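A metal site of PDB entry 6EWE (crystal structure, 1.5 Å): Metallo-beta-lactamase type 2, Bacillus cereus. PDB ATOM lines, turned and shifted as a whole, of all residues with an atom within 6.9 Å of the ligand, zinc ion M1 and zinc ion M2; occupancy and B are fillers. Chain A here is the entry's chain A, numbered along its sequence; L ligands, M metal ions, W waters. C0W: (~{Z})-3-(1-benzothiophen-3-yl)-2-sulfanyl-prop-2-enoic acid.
The side-chain amino group (NZ) of Lys 171 is in salt-bridge range of an oxygen (O) of the ligand (3.7 Å).
The guanidinium group of Arg 91 lies close to the side-chain sulfur of Cys 168 (3.5 Å).
ND1 of His 210 lies within hydrogen-bond range of O of Pro 40 (2.7 Å).
NZ of Lys 171 is in hydrogen-bond range of O of Leu 178 (2.7 Å).
A ring nitrogen (NE2) of His 88 is in hydrogen-bond range of the side-chain carboxylate (OD2) of Asp 183, 2.7 Å away.
The guanidinium group of Arg 91 lies within salt-bridge range of the side-chain carboxylate of Asp 90 (3.6 Å).
The backbone NH (N) of Ala 182 sits at hydrogen-bond distance from the side-chain amide oxygen (OD1) of Asn 180, 2.8 Å away.
Asn 180 touches the ligand (OD1 to C8, 3.2 Å).
OD2 of Asp 183 touches C7 of the ligand, at 3.3 Å.
Hydrophobic or aromatic side chains that line the ligand: His 88, His 149 and His 210.
Of the 24 residues printed, 9 come within 4 Å of the ligand.
Three residues have an atom within 4 Å of zinc ion M1: Asp 90, Cys 168 and His 210.
Within 4 Å of zinc ion M2: His 86, His 88 and His 149.
Along chain A the residues within 4 Å of zinc ion M2 span positions 86 to 149.
Zinc ion M1 is bound by NE2 of His 210, OD2 of Asp 90, O1 of the ligand, S of the ligand and SG of Cys 168.
Zinc ion M1 has five donor atoms within binding distance.
Zinc ion M2 is bound by a ring nitrogen (ND1) of His 88 (2.0 Å), a ring nitrogen (NE2) of His 86 (2.0 Å), a ring nitrogen (NE2) of His 149 (2.1 Å) and a sulfur (S) of the ligand (2.3 Å).
Zinc ion M2 has four donor atoms within binding distance.
Water W2 lies within hydrogen-bond range of O of the ligand (2.5 Å) and N of Asn 180 (2.8 Å).
Water W3 bridges the backbone carbonyl oxygen of Cys 168 (2.9 Å) and the side-chain amino group of Lys 171 (2.9 Å).
Water W1 lies within hydrogen-bond range of the backbone carbonyl oxygen (O) of Asn 180 (2.9 Å), the backbone carbonyl oxygen (O) of His 149 (2.9 Å), the backbone NH (N) of Asp 183 (3.2 Å) and the backbone NH (N) of Ala 184 (3.5 Å).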
ATOM      1  N   PRO A  40     -17.070 -27.489  -0.887  1.00  0.00           N
ATOM      2  CA  PRO A  40     -16.818 -28.838  -1.406  1.00  0.00           C
ATOM      3  C   PRO A  40     -17.135 -28.943  -2.885  1.00  0.00           C
ATOM      4  O   PRO A  40     -17.972 -28.231  -3.426  1.00  0.00           O
ATOM      5  CB  PRO A  40     -17.793 -29.708  -0.597  1.00  0.00           C
ATOM      6  CG  PRO A  40     -18.960 -28.784  -0.373  1.00  0.00           C
ATOM      7  CD  PRO A  40     -18.364 -27.412  -0.181  1.00  0.00           C
ATOM      8  N   SER A  41     -16.393 -29.851  -3.528  1.00  0.00           N
ATOM      9  CA  SER A  41     -16.507 -30.133  -4.941  1.00  0.00           C
ATOM     10  C   SER A  41     -16.489 -31.643  -5.132  1.00  0.00           C
ATOM     11  O   SER A  41     -15.742 -32.342  -4.438  1.00  0.00           O
ATOM     12  CB  SER A  41     -15.283 -29.525  -5.652  1.00  0.00           C
ATOM     13  OG  SER A  41     -15.203 -29.926  -7.001  1.00  0.00           O
ATOM     14  N   TRP A  59      -9.283 -28.767  -6.575  1.00  0.00           N
ATOM     15  CA  TRP A  59      -9.121 -27.314  -6.579  1.00  0.00           C
ATOM     16  C   TRP A  59      -7.675 -26.901  -6.847  1.00  0.00           C
ATOM     17  O   TRP A  59      -7.425 -25.794  -7.335  1.00  0.00           O
ATOM     18  CB  TRP A  59      -9.495 -26.788  -5.200  1.00  0.00           C
ATOM     19  CG  TRP A  59     -10.949 -26.955  -4.839  1.00  0.00           C
ATOM     20  CD1 TRP A  59     -11.511 -27.984  -4.127  1.00  0.00           C
ATOM     21  CD2 TRP A  59     -12.016 -26.051  -5.156  1.00  0.00           C
ATOM     22  NE1 TRP A  59     -12.870 -27.770  -3.989  1.00  0.00           N
ATOM     23  CE2 TRP A  59     -13.203 -26.602  -4.616  1.00  0.00           C
ATOM     24  CE3 TRP A  59     -12.082 -24.833  -5.849  1.00  0.00           C
ATOM     25  CZ2 TRP A  59     -14.433 -25.956  -4.735  1.00  0.00           C
ATOM     26  CZ3 TRP A  59     -13.311 -24.210  -5.962  1.00  0.00           C
ATOM     27  CH2 TRP A  59     -14.470 -24.775  -5.412  1.00  0.00           C
ATOM     28  N   HIS A  86     -14.949 -28.849 -17.239  1.00  0.00           N
ATOM     29  CA  HIS A  86     -14.831 -27.466 -17.718  1.00  0.00           C
ATOM     30  C   HIS A  86     -13.552 -26.863 -17.122  1.00  0.00           C
ATOM     31  O   HIS A  86     -12.812 -27.522 -16.386  1.00  0.00           O
ATOM     32  CB  HIS A  86     -16.105 -26.675 -17.434  1.00  0.00           C
ATOM     33  CG  HIS A  86     -16.355 -26.339 -16.006  1.00  0.00           C
ATOM     34  ND1 HIS A  86     -17.008 -27.179 -15.131  1.00  0.00           N
ATOM     35  CD2 HIS A  86     -16.195 -25.177 -15.344  1.00  0.00           C
ATOM     36  CE1 HIS A  86     -17.165 -26.560 -13.968  1.00  0.00           C
ATOM     37  NE2 HIS A  86     -16.697 -25.337 -14.078  1.00  0.00           N
ATOM     38  N   ALA A  87     -13.217 -25.652 -17.547  1.00  0.00           N
ATOM     39  CA  ALA A  87     -11.925 -25.045 -17.234  1.00  0.00           C
ATOM     40  C   ALA A  87     -11.911 -24.131 -15.990  1.00  0.00           C
ATOM     41  O   ALA A  87     -11.153 -23.169 -15.954  1.00  0.00           O
ATOM     42  CB  ALA A  87     -11.404 -24.297 -18.456  1.00  0.00           C
ATOM     43  N   HIS A  88     -12.716 -24.368 -14.961  1.00  0.00           N
ATOM     44  CA  HIS A  88     -12.546 -23.671 -13.691  1.00  0.00           C
ATOM     45  C   HIS A  88     -11.717 -24.521 -12.728  1.00  0.00           C
ATOM     46  O   HIS A  88     -11.595 -25.726 -12.910  1.00  0.00           O
ATOM     47  CB  HIS A  88     -13.919 -23.465 -13.037  1.00  0.00           C
ATOM     48  CG  HIS A  88     -14.765 -22.376 -13.638  1.00  0.00           C
ATOM     49  ND1 HIS A  88     -16.156 -22.329 -13.496  1.00  0.00           N
ATOM     50  CD2 HIS A  88     -14.433 -21.257 -14.326  1.00  0.00           C
ATOM     51  CE1 HIS A  88     -16.619 -21.249 -14.103  1.00  0.00           C
ATOM     52  NE2 HIS A  88     -15.591 -20.565 -14.581  1.00  0.00           N
ATOM     53  N   ALA A  89     -11.220 -23.864 -11.651  1.00  0.00           N
ATOM     54  CA  ALA A  89     -10.213 -24.453 -10.754  1.00  0.00           C
ATOM     55  C   ALA A  89     -10.698 -25.710 -10.061  1.00  0.00           C
ATOM     56  O   ALA A  89      -9.886 -26.594  -9.747  1.00  0.00           O
ATOM     57  CB  ALA A  89      -9.781 -23.445  -9.669  1.00  0.00           C
ATOM     58  N   ASP A  90     -11.995 -25.808  -9.777  1.00  0.00           N
ATOM     59  CA  ASP A  90     -12.452 -27.008  -9.092  1.00  0.00           C
ATOM     60  C   ASP A  90     -12.335 -28.236  -9.952  1.00  0.00           C
ATOM     61  O   ASP A  90     -12.232 -29.340  -9.422  1.00  0.00           O
ATOM     62  CB  ASP A  90     -13.876 -26.831  -8.540  1.00  0.00           C
ATOM     63  CG  ASP A  90     -14.918 -26.546  -9.587  1.00  0.00           C
ATOM     64  OD1 ASP A  90     -14.617 -25.944 -10.618  1.00  0.00           O
ATOM     65  OD2 ASP A  90     -16.108 -26.895  -9.362  1.00  0.00           O
ATOM     66  N   ARG A  91     -12.345 -28.078 -11.286  1.00  0.00           N
ATOM     67  CA  ARG A  91     -12.250 -29.180 -12.214  1.00  0.00           C
ATOM     68  C   ARG A  91     -10.815 -29.402 -12.647  1.00  0.00           C
ATOM     69  O   ARG A  91     -10.397 -30.542 -12.793  1.00  0.00           O
ATOM     70  CB  ARG A  91     -13.059 -28.915 -13.490  1.00  0.00           C
ATOM     71  CG  ARG A  91     -14.523 -28.455 -13.246  1.00  0.00           C
ATOM     72  CD  ARG A  91     -15.405 -29.559 -12.647  1.00  0.00           C
ATOM     73  NE  ARG A  91     -15.814 -29.253 -11.289  1.00  0.00           N
ATOM     74  CZ  ARG A  91     -16.327 -30.157 -10.468  1.00  0.00           C
ATOM     75  NH1 ARG A  91     -16.541 -31.369 -10.912  1.00  0.00           N
ATOM     76  NH2 ARG A  91     -16.658 -29.817  -9.225  1.00  0.00           N
ATOM     77  N   HIS A 149     -23.552 -23.351 -17.247  1.00  0.00           N
ATOM     78  CA  HIS A 149     -22.677 -22.837 -16.204  1.00  0.00           C
ATOM     79  C   HIS A 149     -21.442 -22.160 -16.779  1.00  0.00           C
ATOM     80  O   HIS A 149     -21.016 -21.122 -16.304  1.00  0.00           O
ATOM     81  CB  HIS A 149     -22.281 -24.016 -15.258  1.00  0.00           C
ATOM     82  CG  HIS A 149     -21.146 -23.690 -14.358  1.00  0.00           C
ATOM     83  ND1 HIS A 149     -21.268 -22.816 -13.334  1.00  0.00           N
ATOM     84  CD2 HIS A 149     -19.844 -24.135 -14.324  1.00  0.00           C
ATOM     85  CE1 HIS A 149     -20.125 -22.691 -12.696  1.00  0.00           C
ATOM     86  NE2 HIS A 149     -19.233 -23.471 -13.303  1.00  0.00           N
ATOM     87  N   THR A 150     -20.896 -22.722 -17.866  1.00  0.00           N
ATOM     88  CA  THR A 150     -19.843 -22.119 -18.632  1.00  0.00           C
ATOM     89  C   THR A 150     -20.095 -22.487 -20.066  1.00  0.00           C
ATOM     90  O   THR A 150     -20.996 -23.252 -20.406  1.00  0.00           O
ATOM     91  CB  THR A 150     -18.457 -22.705 -18.309  1.00  0.00           C
ATOM     92  OG1 THR A 150     -18.476 -24.119 -18.519  1.00  0.00           O
ATOM     93  CG2 THR A 150     -17.955 -22.320 -16.959  1.00  0.00           C
ATOM     94  N   GLY A 167     -21.756 -32.389 -13.231  1.00  0.00           N
ATOM     95  CA  GLY A 167     -20.808 -31.335 -13.035  1.00  0.00           C
ATOM     96  C   GLY A 167     -21.537 -30.089 -12.633  1.00  0.00           C
ATOM     97  O   GLY A 167     -22.635 -30.117 -12.075  1.00  0.00           O
ATOM     98  N   CYS A 168     -20.906 -28.948 -12.936  1.00  0.00           N
ATOM     99  CA  CYS A 168     -21.387 -27.683 -12.431  1.00  0.00           C
ATOM    100  C   CYS A 168     -22.530 -27.143 -13.268  1.00  0.00           C
ATOM    101  O   CYS A 168     -23.174 -26.208 -12.818  1.00  0.00           O
ATOM    102  CB  CYS A 168     -20.195 -26.739 -12.236  1.00  0.00           C
ATOM    103  SG  CYS A 168     -18.955 -27.627 -11.242  1.00  0.00           S
ATOM    104  N   LEU A 169     -22.870 -27.816 -14.376  1.00  0.00           N
ATOM    105  CA  LEU A 169     -24.126 -27.591 -15.078  1.00  0.00           C
ATOM    106  C   LEU A 169     -25.342 -27.897 -14.202  1.00  0.00           C
ATOM    107  O   LEU A 169     -26.420 -27.324 -14.415  1.00  0.00           O
ATOM    108  CB  LEU A 169     -24.157 -28.481 -16.332  1.00  0.00           C
ATOM    109  CG  LEU A 169     -25.341 -28.299 -17.253  1.00  0.00           C
ATOM    110  CD1 LEU A 169     -25.184 -26.969 -18.038  1.00  0.00           C
ATOM    111  CD2 LEU A 169     -25.446 -29.466 -18.200  1.00  0.00           C
ATOM    112  N   LYS A 171     -27.163 -28.204 -10.475  1.00  0.00           N
ATOM    113  CA  LYS A 171     -27.142 -27.740  -9.094  1.00  0.00           C
ATOM    114  C   LYS A 171     -27.729 -28.800  -8.169  1.00  0.00           C
ATOM    115  O   LYS A 171     -28.657 -29.517  -8.536  1.00  0.00           O
ATOM    116  CB  LYS A 171     -27.964 -26.446  -8.967  1.00  0.00           C
ATOM    117  CG  LYS A 171     -27.341 -25.273  -9.693  1.00  0.00           C
ATOM    118  CD  LYS A 171     -26.019 -24.892  -9.075  1.00  0.00           C
ATOM    119  CE  LYS A 171     -25.337 -23.760  -9.814  1.00  0.00           C
ATOM    120  NZ  LYS A 171     -24.060 -23.387  -9.077  1.00  0.00           N
ATOM    121  N   LEU A 178     -27.974 -19.886  -8.626  1.00  0.00           N
ATOM    122  CA  LEU A 178     -27.114 -20.501  -9.644  1.00  0.00           C
ATOM    123  C   LEU A 178     -25.631 -20.376  -9.341  1.00  0.00           C
ATOM    124  O   LEU A 178     -24.808 -20.951 -10.085  1.00  0.00           O
ATOM    125  CB  LEU A 178     -27.427 -19.864 -11.002  1.00  0.00           C
ATOM    126  CG  LEU A 178     -28.818 -20.129 -11.539  1.00  0.00           C
ATOM    127  CD1 LEU A 178     -29.130 -19.192 -12.726  1.00  0.00           C
ATOM    128  CD2 LEU A 178     -28.969 -21.590 -11.935  1.00  0.00           C
ATOM    129  N   GLY A 179     -25.266 -19.651  -8.277  1.00  0.00           N
ATOM    130  CA  GLY A 179     -23.862 -19.413  -7.940  1.00  0.00           C
ATOM    131  C   GLY A 179     -23.263 -18.294  -8.779  1.00  0.00           C
ATOM    132  O   GLY A 179     -23.954 -17.395  -9.232  1.00  0.00           O
ATOM    133  N   ASN A 180     -21.958 -18.374  -9.001  1.00  0.00           N
ATOM    134  CA  ASN A 180     -21.261 -17.364  -9.803  1.00  0.00           C
ATOM    135  C   ASN A 180     -21.591 -17.616 -11.263  1.00  0.00           C
ATOM    136  O   ASN A 180     -21.280 -18.679 -11.802  1.00  0.00           O
ATOM    137  CB  ASN A 180     -19.745 -17.393  -9.543  1.00  0.00           C
ATOM    138  CG  ASN A 180     -19.018 -16.199 -10.188  1.00  0.00           C
ATOM    139  OD1 ASN A 180     -19.412 -15.737 -11.237  1.00  0.00           O
ATOM    140  ND2 ASN A 180     -17.958 -15.710  -9.543  1.00  0.00           N
ATOM    141  N   VAL A 181     -22.279 -16.638 -11.871  1.00  0.00           N
ATOM    142  CA  VAL A 181     -22.716 -16.711 -13.253  1.00  0.00           C
ATOM    143  C   VAL A 181     -21.871 -15.837 -14.164  1.00  0.00           C
ATOM    144  O   VAL A 181     -22.252 -15.606 -15.309  1.00  0.00           O
ATOM    145  CB  VAL A 181     -24.226 -16.408 -13.379  1.00  0.00           C
ATOM    146  CG1 VAL A 181     -25.003 -17.515 -12.693  1.00  0.00           C
ATOM    147  CG2 VAL A 181     -24.588 -14.965 -12.821  1.00  0.00           C
ATOM    148  N   ALA A 182     -20.695 -15.381 -13.699  1.00  0.00           N
ATOM    149  CA  ALA A 182     -19.864 -14.509 -14.529  1.00  0.00           C
ATOM    150  C   ALA A 182     -19.500 -15.176 -15.853  1.00  0.00           C
ATOM    151  O   ALA A 182     -19.427 -14.497 -16.893  1.00  0.00           O
ATOM    152  CB  ALA A 182     -18.584 -14.092 -13.788  1.00  0.00           C
ATOM    153  N   ASP A 183     -19.267 -16.492 -15.844  1.00  0.00           N
ATOM    154  CA  ASP A 183     -18.898 -17.222 -17.046  1.00  0.00           C
ATOM    155  C   ASP A 183     -20.070 -17.963 -17.655  1.00  0.00           C
ATOM    156  O   ASP A 183     -19.877 -18.777 -18.542  1.00  0.00           O
ATOM    157  CB  ASP A 183     -17.745 -18.223 -16.765  1.00  0.00           C
ATOM    158  CG  ASP A 183     -16.437 -17.535 -16.416  1.00  0.00           C
ATOM    159  OD1 ASP A 183     -16.283 -16.319 -16.701  1.00  0.00           O
ATOM    160  OD2 ASP A 183     -15.537 -18.236 -15.893  1.00  0.00           O
ATOM    161  N   ALA A 184     -21.307 -17.688 -17.194  1.00  0.00           N
ATOM    162  CA  ALA A 184     -22.462 -18.508 -17.502  1.00  0.00           C
ATOM    163  C   ALA A 184     -23.311 -17.900 -18.619  1.00  0.00           C
ATOM    164  O   ALA A 184     -23.160 -16.720 -18.985  1.00  0.00           O
ATOM    165  CB  ALA A 184     -23.323 -18.688 -16.246  1.00  0.00           C
ATOM    166  N   GLY A 209     -21.844 -30.958  -9.464  1.00  0.00           N
ATOM    167  CA  GLY A 209     -20.471 -30.511  -9.203  1.00  0.00           C
ATOM    168  C   GLY A 209     -20.204 -30.200  -7.744  1.00  0.00           C
ATOM    169  O   GLY A 209     -19.072 -30.350  -7.264  1.00  0.00           O
ATOM    170  N   HIS A 210     -21.219 -29.790  -7.021  1.00  0.00           N
ATOM    171  CA  HIS A 210     -21.152 -29.448  -5.604  1.00  0.00           C
ATOM    172  C   HIS A 210     -22.441 -29.932  -4.949  1.00  0.00           C
ATOM    173  O   HIS A 210     -23.535 -29.710  -5.483  1.00  0.00           O
ATOM    174  CB  HIS A 210     -20.956 -27.925  -5.415  1.00  0.00           C
ATOM    175  CG  HIS A 210     -19.865 -27.341  -6.288  1.00  0.00           C
ATOM    176  ND1 HIS A 210     -18.571 -27.199  -5.864  1.00  0.00           N
ATOM    177  CD2 HIS A 210     -19.913 -26.837  -7.554  1.00  0.00           C
ATOM    178  CE1 HIS A 210     -17.838 -26.675  -6.842  1.00  0.00           C
ATOM    179  NE2 HIS A 210     -18.633 -26.423  -7.871  1.00  0.00           N
HETATM  180  C4  C0W L   1     -15.447 -21.249  -9.920  1.00  0.00           C
HETATM  181  C5  C0W L   1     -15.368 -19.189 -11.316  1.00  0.00           C
HETATM  182  C6  C0W L   1     -15.108 -18.075 -12.103  1.00  0.00           C
HETATM  183  C7  C0W L   1     -16.154 -17.433 -12.723  1.00  0.00           C
HETATM  184  C8  C0W L   1     -17.454 -17.889 -12.558  1.00  0.00           C
HETATM  185  C9  C0W L   1     -17.716 -18.981 -11.747  1.00  0.00           C
HETATM  186  C10 C0W L   1     -16.679 -19.659 -11.105  1.00  0.00           C
HETATM  187  C   C0W L   1     -19.550 -23.457  -9.640  1.00  0.00           C
HETATM  188  O   C0W L   1     -20.421 -22.592  -9.116  1.00  0.00           O
HETATM  189  C1  C0W L   1     -18.222 -22.907  -9.971  1.00  0.00           C
HETATM  190  C2  C0W L   1     -17.932 -21.577  -9.958  1.00  0.00           C
HETATM  191  C3  C0W L   1     -16.709 -20.856 -10.291  1.00  0.00           C
HETATM  192  O1  C0W L   1     -19.821 -24.597  -9.884  1.00  0.00           O
HETATM  193  S   C0W L   1     -16.994 -24.075 -10.494  1.00  0.00           S
HETATM  194  S1  C0W L   1     -14.202 -20.222 -10.528  1.00  0.00           S
HETATM  195 ZN    ZN M   1     -18.033 -25.991  -9.826  1.00  0.00          ZN
HETATM  196 ZN    ZN M   2     -17.264 -23.868 -12.783  1.00  0.00          ZN
HETATM  197  O   HOH W   1     -19.989 -19.197 -14.350  1.00  0.00           O
HETATM  198  O   HOH W   2     -20.496 -20.452  -7.785  1.00  0.00           O
HETATM  199  O   HOH W   3     -22.476 -25.573 -10.116  1.00  0.00           O
